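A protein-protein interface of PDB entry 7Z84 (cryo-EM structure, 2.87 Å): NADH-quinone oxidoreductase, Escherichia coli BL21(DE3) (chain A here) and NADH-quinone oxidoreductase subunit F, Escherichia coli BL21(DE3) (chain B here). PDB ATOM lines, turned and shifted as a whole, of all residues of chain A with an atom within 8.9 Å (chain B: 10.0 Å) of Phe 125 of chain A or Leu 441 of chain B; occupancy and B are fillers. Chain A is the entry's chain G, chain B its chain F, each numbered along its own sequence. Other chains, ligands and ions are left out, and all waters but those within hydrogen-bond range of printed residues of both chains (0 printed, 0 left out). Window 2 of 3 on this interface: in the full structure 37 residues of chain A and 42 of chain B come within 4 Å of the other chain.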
ATOM      1  N   GLU A  89      20.805  -7.198 -13.172  1.00  0.00           N
ATOM      2  CA  GLU A  89      21.855  -7.086 -14.179  1.00  0.00           C
ATOM      3  C   GLU A  89      21.328  -7.424 -15.569  1.00  0.00           C
ATOM      4  O   GLU A  89      21.719  -6.792 -16.555  1.00  0.00           O
ATOM      5  CB  GLU A  89      23.033  -7.986 -13.810  1.00  0.00           C
ATOM      6  CG  GLU A  89      24.248  -7.804 -14.699  1.00  0.00           C
ATOM      7  CD  GLU A  89      25.412  -8.672 -14.278  1.00  0.00           C
ATOM      8  OE1 GLU A  89      25.269  -9.420 -13.288  1.00  0.00           O
ATOM      9  OE2 GLU A  89      26.470  -8.609 -14.939  1.00  0.00           O
ATOM     10  N   VAL A  92      19.373  -4.368 -16.816  1.00  0.00           N
ATOM     11  CA  VAL A  92      20.320  -3.359 -17.293  1.00  0.00           C
ATOM     12  C   VAL A  92      20.908  -3.769 -18.642  1.00  0.00           C
ATOM     13  O   VAL A  92      21.037  -2.943 -19.555  1.00  0.00           O
ATOM     14  CB  VAL A  92      21.414  -3.112 -16.234  1.00  0.00           C
ATOM     15  CG1 VAL A  92      22.695  -2.591 -16.862  1.00  0.00           C
ATOM     16  CG2 VAL A  92      20.922  -2.125 -15.203  1.00  0.00           C
ATOM     17  N   GLU A  93      21.229  -5.056 -18.801  1.00  0.00           N
ATOM     18  CA  GLU A  93      21.768  -5.556 -20.063  1.00  0.00           C
ATOM     19  C   GLU A  93      20.767  -5.411 -21.205  1.00  0.00           C
ATOM     20  O   GLU A  93      21.140  -5.015 -22.314  1.00  0.00           O
ATOM     21  CB  GLU A  93      22.186  -7.015 -19.901  1.00  0.00           C
ATOM     22  CG  GLU A  93      22.754  -7.645 -21.151  1.00  0.00           C
ATOM     23  CD  GLU A  93      23.334  -9.016 -20.891  1.00  0.00           C
ATOM     24  OE1 GLU A  93      22.901  -9.670 -19.920  1.00  0.00           O
ATOM     25  OE2 GLU A  93      24.227  -9.437 -21.652  1.00  0.00           O
ATOM     26  N   MET A  96      20.651  -2.064 -22.292  1.00  0.00           N
ATOM     27  CA  MET A  96      21.902  -1.686 -22.929  1.00  0.00           C
ATOM     28  C   MET A  96      22.076  -2.296 -24.313  1.00  0.00           C
ATOM     29  O   MET A  96      23.085  -2.022 -24.968  1.00  0.00           O
ATOM     30  CB  MET A  96      23.084  -2.085 -22.043  1.00  0.00           C
ATOM     31  CG  MET A  96      23.328  -1.082 -20.950  1.00  0.00           C
ATOM     32  SD  MET A  96      24.372   0.266 -21.473  1.00  0.00           S
ATOM     33  CE  MET A  96      23.169   1.576 -21.283  1.00  0.00           C
ATOM     34  N   THR A 118      23.801   1.175 -14.305  1.00  0.00           N
ATOM     35  CA  THR A 118      24.633   0.202 -15.003  1.00  0.00           C
ATOM     36  C   THR A 118      25.846  -0.175 -14.166  1.00  0.00           C
ATOM     37  O   THR A 118      26.217  -1.351 -14.096  1.00  0.00           O
ATOM     38  CB  THR A 118      25.070   0.758 -16.358  1.00  0.00           C
ATOM     39  OG1 THR A 118      23.946   1.344 -17.024  1.00  0.00           O
ATOM     40  CG2 THR A 118      25.646  -0.341 -17.230  1.00  0.00           C
ATOM     41  N   GLY A 122      26.519  -3.840 -11.699  1.00  0.00           N
ATOM     42  CA  GLY A 122      27.714  -4.594 -12.006  1.00  0.00           C
ATOM     43  C   GLY A 122      27.792  -5.118 -13.417  1.00  0.00           C
ATOM     44  O   GLY A 122      28.486  -6.109 -13.659  1.00  0.00           O
ATOM     45  N   HIS A 123      27.101  -4.486 -14.361  1.00  0.00           N
ATOM     46  CA  HIS A 123      27.083  -4.928 -15.749  1.00  0.00           C
ATOM     47  C   HIS A 123      28.116  -4.128 -16.531  1.00  0.00           C
ATOM     48  O   HIS A 123      27.940  -2.926 -16.757  1.00  0.00           O
ATOM     49  CB  HIS A 123      25.694  -4.762 -16.356  1.00  0.00           C
ATOM     50  CG  HIS A 123      25.618  -5.164 -17.793  1.00  0.00           C
ATOM     51  ND1 HIS A 123      25.780  -6.468 -18.207  1.00  0.00           N
ATOM     52  CD2 HIS A 123      25.412  -4.436 -18.915  1.00  0.00           C
ATOM     53  CE1 HIS A 123      25.669  -6.527 -19.521  1.00  0.00           C
ATOM     54  NE2 HIS A 123      25.447  -5.307 -19.976  1.00  0.00           N
ATOM     55  N   SER A 124      29.191  -4.796 -16.946  1.00  0.00           N
ATOM     56  CA  SER A 124      30.248  -4.142 -17.701  1.00  0.00           C
ATOM     57  C   SER A 124      30.731  -4.949 -18.897  1.00  0.00           C
ATOM     58  O   SER A 124      31.631  -4.487 -19.602  1.00  0.00           O
ATOM     59  CB  SER A 124      31.442  -3.830 -16.786  1.00  0.00           C
ATOM     60  OG  SER A 124      31.822  -4.970 -16.037  1.00  0.00           O
ATOM     61  N   PHE A 125      30.167  -6.127 -19.151  1.00  0.00           N
ATOM     62  CA  PHE A 125      30.564  -6.977 -20.263  1.00  0.00           C
ATOM     63  C   PHE A 125      29.401  -7.095 -21.236  1.00  0.00           C
ATOM     64  O   PHE A 125      28.297  -7.481 -20.842  1.00  0.00           O
ATOM     65  CB  PHE A 125      30.986  -8.363 -19.768  1.00  0.00           C
ATOM     66  CG  PHE A 125      31.738  -9.169 -20.785  1.00  0.00           C
ATOM     67  CD1 PHE A 125      33.114  -9.056 -20.894  1.00  0.00           C
ATOM     68  CD2 PHE A 125      31.072 -10.048 -21.626  1.00  0.00           C
ATOM     69  CE1 PHE A 125      33.812  -9.797 -21.827  1.00  0.00           C
ATOM     70  CE2 PHE A 125      31.764 -10.791 -22.563  1.00  0.00           C
ATOM     71  CZ  PHE A 125      33.135 -10.666 -22.662  1.00  0.00           C
ATOM     72  N   ARG A 126      29.653  -6.777 -22.501  1.00  0.00           N
ATOM     73  CA  ARG A 126      28.638  -6.849 -23.544  1.00  0.00           C
ATOM     74  C   ARG A 126      28.815  -8.135 -24.338  1.00  0.00           C
ATOM     75  O   ARG A 126      29.892  -8.389 -24.885  1.00  0.00           O
ATOM     76  CB  ARG A 126      28.718  -5.639 -24.473  1.00  0.00           C
ATOM     77  CG  ARG A 126      27.602  -5.565 -25.500  1.00  0.00           C
ATOM     78  CD  ARG A 126      27.729  -4.317 -26.357  1.00  0.00           C
ATOM     79  NE  ARG A 126      26.642  -4.185 -27.319  1.00  0.00           N
ATOM     80  CZ  ARG A 126      25.510  -3.535 -27.092  1.00  0.00           C
ATOM     81  NH1 ARG A 126      25.268  -2.954 -25.930  1.00  0.00           N
ATOM     82  NH2 ARG A 126      24.597  -3.469 -28.054  1.00  0.00           N
ATOM     83  N   ARG A 127      27.759  -8.941 -24.398  1.00  0.00           N
ATOM     84  CA  ARG A 127      27.725 -10.118 -25.250  1.00  0.00           C
ATOM     85  C   ARG A 127      26.674 -10.028 -26.345  1.00  0.00           C
ATOM     86  O   ARG A 127      26.631 -10.907 -27.211  1.00  0.00           O
ATOM     87  CB  ARG A 127      27.485 -11.376 -24.407  1.00  0.00           C
ATOM     88  CG  ARG A 127      26.335 -11.232 -23.447  1.00  0.00           C
ATOM     89  CD  ARG A 127      26.576 -12.027 -22.183  1.00  0.00           C
ATOM     90  NE  ARG A 127      25.383 -12.054 -21.350  1.00  0.00           N
ATOM     91  CZ  ARG A 127      24.379 -12.905 -21.501  1.00  0.00           C
ATOM     92  NH1 ARG A 127      24.403 -13.847 -22.429  1.00  0.00           N
ATOM     93  NH2 ARG A 127      23.320 -12.803 -20.706  1.00  0.00           N
ATOM     94  N   TYR A 128      25.829  -9.002 -26.322  1.00  0.00           N
ATOM     95  CA  TYR A 128      24.923  -8.738 -27.430  1.00  0.00           C
ATOM     96  C   TYR A 128      25.728  -8.305 -28.649  1.00  0.00           C
ATOM     97  O   TYR A 128      26.541  -7.380 -28.572  1.00  0.00           O
ATOM     98  CB  TYR A 128      23.916  -7.660 -27.030  1.00  0.00           C
ATOM     99  CG  TYR A 128      22.864  -7.330 -28.065  1.00  0.00           C
ATOM    100  CD1 TYR A 128      21.699  -8.079 -28.167  1.00  0.00           C
ATOM    101  CD2 TYR A 128      23.020  -6.248 -28.918  1.00  0.00           C
ATOM    102  CE1 TYR A 128      20.732  -7.770 -29.103  1.00  0.00           C
ATOM    103  CE2 TYR A 128      22.061  -5.932 -29.857  1.00  0.00           C
ATOM    104  CZ  TYR A 128      20.920  -6.694 -29.944  1.00  0.00           C
ATOM    105  OH  TYR A 128      19.965  -6.375 -30.879  1.00  0.00           O
ATOM    106  N   TRP B 363      15.952  -9.940 -28.748  1.00  0.00           N
ATOM    107  CA  TRP B 363      17.227 -10.642 -28.624  1.00  0.00           C
ATOM    108  C   TRP B 363      17.070 -12.123 -28.942  1.00  0.00           C
ATOM    109  O   TRP B 363      17.898 -12.703 -29.655  1.00  0.00           O
ATOM    110  CB  TRP B 363      17.801 -10.452 -27.219  1.00  0.00           C
ATOM    111  CG  TRP B 363      19.274 -10.759 -27.105  1.00  0.00           C
ATOM    112  CD1 TRP B 363      20.096 -11.235 -28.085  1.00  0.00           C
ATOM    113  CD2 TRP B 363      20.092 -10.612 -25.939  1.00  0.00           C
ATOM    114  NE1 TRP B 363      21.369 -11.390 -27.605  1.00  0.00           N
ATOM    115  CE2 TRP B 363      21.394 -11.014 -26.288  1.00  0.00           C
ATOM    116  CE3 TRP B 363      19.848 -10.175 -24.634  1.00  0.00           C
ATOM    117  CZ2 TRP B 363      22.449 -10.995 -25.381  1.00  0.00           C
ATOM    118  CZ3 TRP B 363      20.897 -10.156 -23.736  1.00  0.00           C
ATOM    119  CH2 TRP B 363      22.181 -10.564 -24.113  1.00  0.00           C
ATOM    120  N   PRO B 378      28.849 -19.524 -29.845  1.00  0.00           N
ATOM    121  CA  PRO B 378      28.721 -20.135 -28.514  1.00  0.00           C
ATOM    122  C   PRO B 378      28.153 -19.174 -27.480  1.00  0.00           C
ATOM    123  O   PRO B 378      28.439 -17.976 -27.489  1.00  0.00           O
ATOM    124  CB  PRO B 378      30.160 -20.536 -28.173  1.00  0.00           C
ATOM    125  CG  PRO B 378      30.792 -20.766 -29.489  1.00  0.00           C
ATOM    126  CD  PRO B 378      30.192 -19.743 -30.410  1.00  0.00           C
ATOM    127  N   GLN B 386      18.563 -18.274 -20.345  1.00  0.00           N
ATOM    128  CA  GLN B 386      18.436 -17.191 -19.376  1.00  0.00           C
ATOM    129  C   GLN B 386      17.265 -16.274 -19.714  1.00  0.00           C
ATOM    130  O   GLN B 386      16.607 -15.742 -18.812  1.00  0.00           O
ATOM    131  CB  GLN B 386      19.736 -16.398 -19.293  1.00  0.00           C
ATOM    132  CG  GLN B 386      20.050 -15.916 -17.889  1.00  0.00           C
ATOM    133  CD  GLN B 386      21.167 -14.906 -17.860  1.00  0.00           C
ATOM    134  OE1 GLN B 386      21.485 -14.280 -18.871  1.00  0.00           O
ATOM    135  NE2 GLN B 386      21.782 -14.748 -16.701  1.00  0.00           N
ATOM    136  N   PHE B 427      32.480 -17.291 -31.235  1.00  0.00           N
ATOM    137  CA  PHE B 427      31.909 -16.089 -30.640  1.00  0.00           C
ATOM    138  C   PHE B 427      32.787 -14.879 -30.928  1.00  0.00           C
ATOM    139  O   PHE B 427      33.986 -14.881 -30.635  1.00  0.00           O
ATOM    140  CB  PHE B 427      31.731 -16.256 -29.133  1.00  0.00           C
ATOM    141  CG  PHE B 427      31.171 -15.038 -28.459  1.00  0.00           C
ATOM    142  CD1 PHE B 427      29.862 -14.642 -28.694  1.00  0.00           C
ATOM    143  CD2 PHE B 427      31.950 -14.279 -27.601  1.00  0.00           C
ATOM    144  CE1 PHE B 427      29.340 -13.518 -28.083  1.00  0.00           C
ATOM    145  CE2 PHE B 427      31.434 -13.152 -26.985  1.00  0.00           C
ATOM    146  CZ  PHE B 427      30.127 -12.772 -27.226  1.00  0.00           C
ATOM    147  N   SER B 428      32.183 -13.842 -31.502  1.00  0.00           N
ATOM    148  CA  SER B 428      32.891 -12.609 -31.835  1.00  0.00           C
ATOM    149  C   SER B 428      31.946 -11.439 -31.613  1.00  0.00           C
ATOM    150  O   SER B 428      30.968 -11.278 -32.350  1.00  0.00           O
ATOM    151  CB  SER B 428      33.397 -12.632 -33.277  1.00  0.00           C
ATOM    152  OG  SER B 428      33.933 -11.374 -33.645  1.00  0.00           O
ATOM    153  N   ASN B 429      32.237 -10.625 -30.600  1.00  0.00           N
ATOM    154  CA  ASN B 429      31.491  -9.403 -30.347  1.00  0.00           C
ATOM    155  C   ASN B 429      32.278  -8.143 -30.657  1.00  0.00           C
ATOM    156  O   ASN B 429      31.671  -7.121 -30.991  1.00  0.00           O
ATOM    157  CB  ASN B 429      31.037  -9.346 -28.882  1.00  0.00           C
ATOM    158  CG  ASN B 429      29.842  -8.448 -28.683  1.00  0.00           C
ATOM    159  OD1 ASN B 429      29.232  -7.989 -29.646  1.00  0.00           O
ATOM    160  ND2 ASN B 429      29.509  -8.177 -27.432  1.00  0.00           N
ATOM    161  N   THR B 430      33.602  -8.192 -30.564  1.00  0.00           N
ATOM    162  CA  THR B 430      34.456  -7.043 -30.802  1.00  0.00           C
ATOM    163  C   THR B 430      35.246  -7.238 -32.087  1.00  0.00           C
ATOM    164  O   THR B 430      35.578  -8.363 -32.468  1.00  0.00           O
ATOM    165  CB  THR B 430      35.434  -6.828 -29.641  1.00  0.00           C
ATOM    166  OG1 THR B 430      36.512  -7.766 -29.747  1.00  0.00           O
ATOM    167  CG2 THR B 430      34.743  -7.031 -28.312  1.00  0.00           C
ATOM    168  N   GLN B 437      46.136  -3.701 -27.548  1.00  0.00           N
ATOM    169  CA  GLN B 437      46.155  -5.146 -27.365  1.00  0.00           C
ATOM    170  C   GLN B 437      44.930  -5.580 -26.568  1.00  0.00           C
ATOM    171  O   GLN B 437      44.685  -5.046 -25.483  1.00  0.00           O
ATOM    172  CB  GLN B 437      47.431  -5.583 -26.656  1.00  0.00           C
ATOM    173  CG  GLN B 437      48.648  -5.618 -27.561  1.00  0.00           C
ATOM    174  CD  GLN B 437      49.953  -5.582 -26.793  1.00  0.00           C
ATOM    175  OE1 GLN B 437      50.324  -4.555 -26.227  1.00  0.00           O
ATOM    176  NE2 GLN B 437      50.660  -6.704 -26.774  1.00  0.00           N
ATOM    177  N   PRO B 438      44.142  -6.526 -27.071  1.00  0.00           N
ATOM    178  CA  PRO B 438      42.900  -6.894 -26.386  1.00  0.00           C
ATOM    179  C   PRO B 438      43.156  -7.732 -25.143  1.00  0.00           C
ATOM    180  O   PRO B 438      44.221  -8.323 -24.957  1.00  0.00           O
ATOM    181  CB  PRO B 438      42.141  -7.697 -27.446  1.00  0.00           C
ATOM    182  CG  PRO B 438      43.218  -8.301 -28.276  1.00  0.00           C
ATOM    183  CD  PRO B 438      44.346  -7.305 -28.304  1.00  0.00           C
ATOM    184  N   ASN B 439      42.144  -7.767 -24.280  1.00  0.00           N
ATOM    185  CA  ASN B 439      42.178  -8.579 -23.065  1.00  0.00           C
ATOM    186  C   ASN B 439      41.756  -9.995 -23.433  1.00  0.00           C
ATOM    187  O   ASN B 439      40.573 -10.271 -23.641  1.00  0.00           O
ATOM    188  CB  ASN B 439      41.266  -7.984 -21.999  1.00  0.00           C
ATOM    189  CG  ASN B 439      41.698  -8.347 -20.595  1.00  0.00           C
ATOM    190  OD1 ASN B 439      42.889  -8.433 -20.302  1.00  0.00           O
ATOM    191  ND2 ASN B 439      40.727  -8.564 -19.715  1.00  0.00           N
ATOM    192  N   LEU B 440      42.730 -10.900 -23.514  1.00  0.00           N
ATOM    193  CA  LEU B 440      42.492 -12.269 -23.969  1.00  0.00           C
ATOM    194  C   LEU B 440      41.959 -13.091 -22.801  1.00  0.00           C
ATOM    195  O   LEU B 440      42.694 -13.774 -22.083  1.00  0.00           O
ATOM    196  CB  LEU B 440      43.770 -12.869 -24.541  1.00  0.00           C
ATOM    197  CG  LEU B 440      44.419 -12.081 -25.677  1.00  0.00           C
ATOM    198  CD1 LEU B 440      45.818 -12.604 -25.962  1.00  0.00           C
ATOM    199  CD2 LEU B 440      43.555 -12.134 -26.924  1.00  0.00           C
ATOM    200  N   LEU B 441      40.642 -13.027 -22.616  1.00  0.00           N
ATOM    201  CA  LEU B 441      39.996 -13.740 -21.522  1.00  0.00           C
ATOM    202  C   LEU B 441      39.967 -15.235 -21.817  1.00  0.00           C
ATOM    203  O   LEU B 441      39.331 -15.673 -22.781  1.00  0.00           O
ATOM    204  CB  LEU B 441      38.581 -13.210 -21.309  1.00  0.00           C
ATOM    205  CG  LEU B 441      38.449 -11.886 -20.555  1.00  0.00           C
ATOM    206  CD1 LEU B 441      37.066 -11.297 -20.764  1.00  0.00           C
ATOM    207  CD2 LEU B 441      38.736 -12.077 -19.076  1.00  0.00           C
ATOM    208  N   LYS B 442      40.653 -16.015 -20.988  1.00  0.00           N
ATOM    209  CA  LYS B 442      40.694 -17.463 -21.151  1.00  0.00           C
ATOM    210  C   LYS B 442      39.515 -18.126 -20.445  1.00  0.00           C
ATOM    211  O   LYS B 442      39.628 -19.244 -19.942  1.00  0.00           O
ATOM    212  CB  LYS B 442      42.012 -18.027 -20.617  1.00  0.00           C
ATOM    213  CG  LYS B 442      43.239 -17.587 -21.395  1.00  0.00           C
ATOM    214  CD  LYS B 442      43.303 -18.258 -22.756  1.00  0.00           C
ATOM    215  CE  LYS B 442      44.617 -17.954 -23.460  1.00  0.00           C
ATOM    216  NZ  LYS B 442      44.663 -16.561 -23.983  1.00  0.00           N
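O of Tyr 128 of chain A lies within hydrogen-bond range of NE of Arg 126 of chain A (3.4 Å). The backbone carbonyl oxygen (O) of Met 96 of chain A lies within hydrogen-bond range of the guanidinium group (NH1) of Arg 126 of chain A, at 2.6 Å. The side-chain carboxylate of Glu 93 of chain A is in salt-bridge range of the guanidinium group of Arg 127 of chain A (2.9 Å).
ND2 of Asn 429 of chain B sits at hydrogen-bond distance from O of Arg 126 of chain A, 2.6 Å away. The side-chain amide oxygen of Gln 386 of chain B sits at hydrogen-bond distance from the guanidinium group of Arg 127 of chain A (3.0 Å). The side-chain amide oxygen (OD1) of Asn 429 of chain B lies close to the backbone carbonyl oxygen (O) of Tyr 128 of chain A, 3.0 Å away.
Among the printed residues, pairs that only touch across the chains: Glu 93 of chain A with Trp 363 of chain B, Phe 125 of chain A with Leu 441 of chain B, Arg 127 of chain A with Phe 427 of chain B, Arg 127 of chain A with Asn 429 of chain B and Tyr 128 of chain A with Trp 363 of chain B.
Of the 13 printed residues of chain B, 5 touch a printed residue of chain A. Hydrophobic or aromatic side chains of chain B that line the printed part of chain A: Trp 363, Phe 427 and Leu 441. Of the 12 printed residues of chain A, 5 touch a printed residue of chain B. Hydrophobic or aromatic side chains of chain A that line the printed part of chain B: Phe 125 and Tyr 128. Along chain A the printed residues that touch a printed residue of chain B span positions 93 to 128.
No residue of chain B comes within 4 Å of Ser 124 of chain A. Printed residues of chain B within 4 Å of Phe 125 of chain A: Leu 441 (3.7 Å). Of the printed residues of chain B, Arg 126 of chain A touches Asn 429 (2.6 Å). Of the printed residues of chain A, Trp 363 of chain B touches Glu 93 (3.4 Å) and Tyr 128 (3.4 Å). Printed residues of chain A within 4 Å of Gln 386 of chain B: Arg 127. Of the printed residues of chain A, Asn 429 of chain B touches Arg 126 (2.6 Å), Arg 127 (3.4 Å) and Tyr 128 (3.0 Å). Leu 441 of chain B touches just one residue of chain A: Phe 125 (3.7 Å). The nearest printed residue of chain B that does not touch Arg 126 of chain A is Phe 427 of chain B (5.0 Å).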
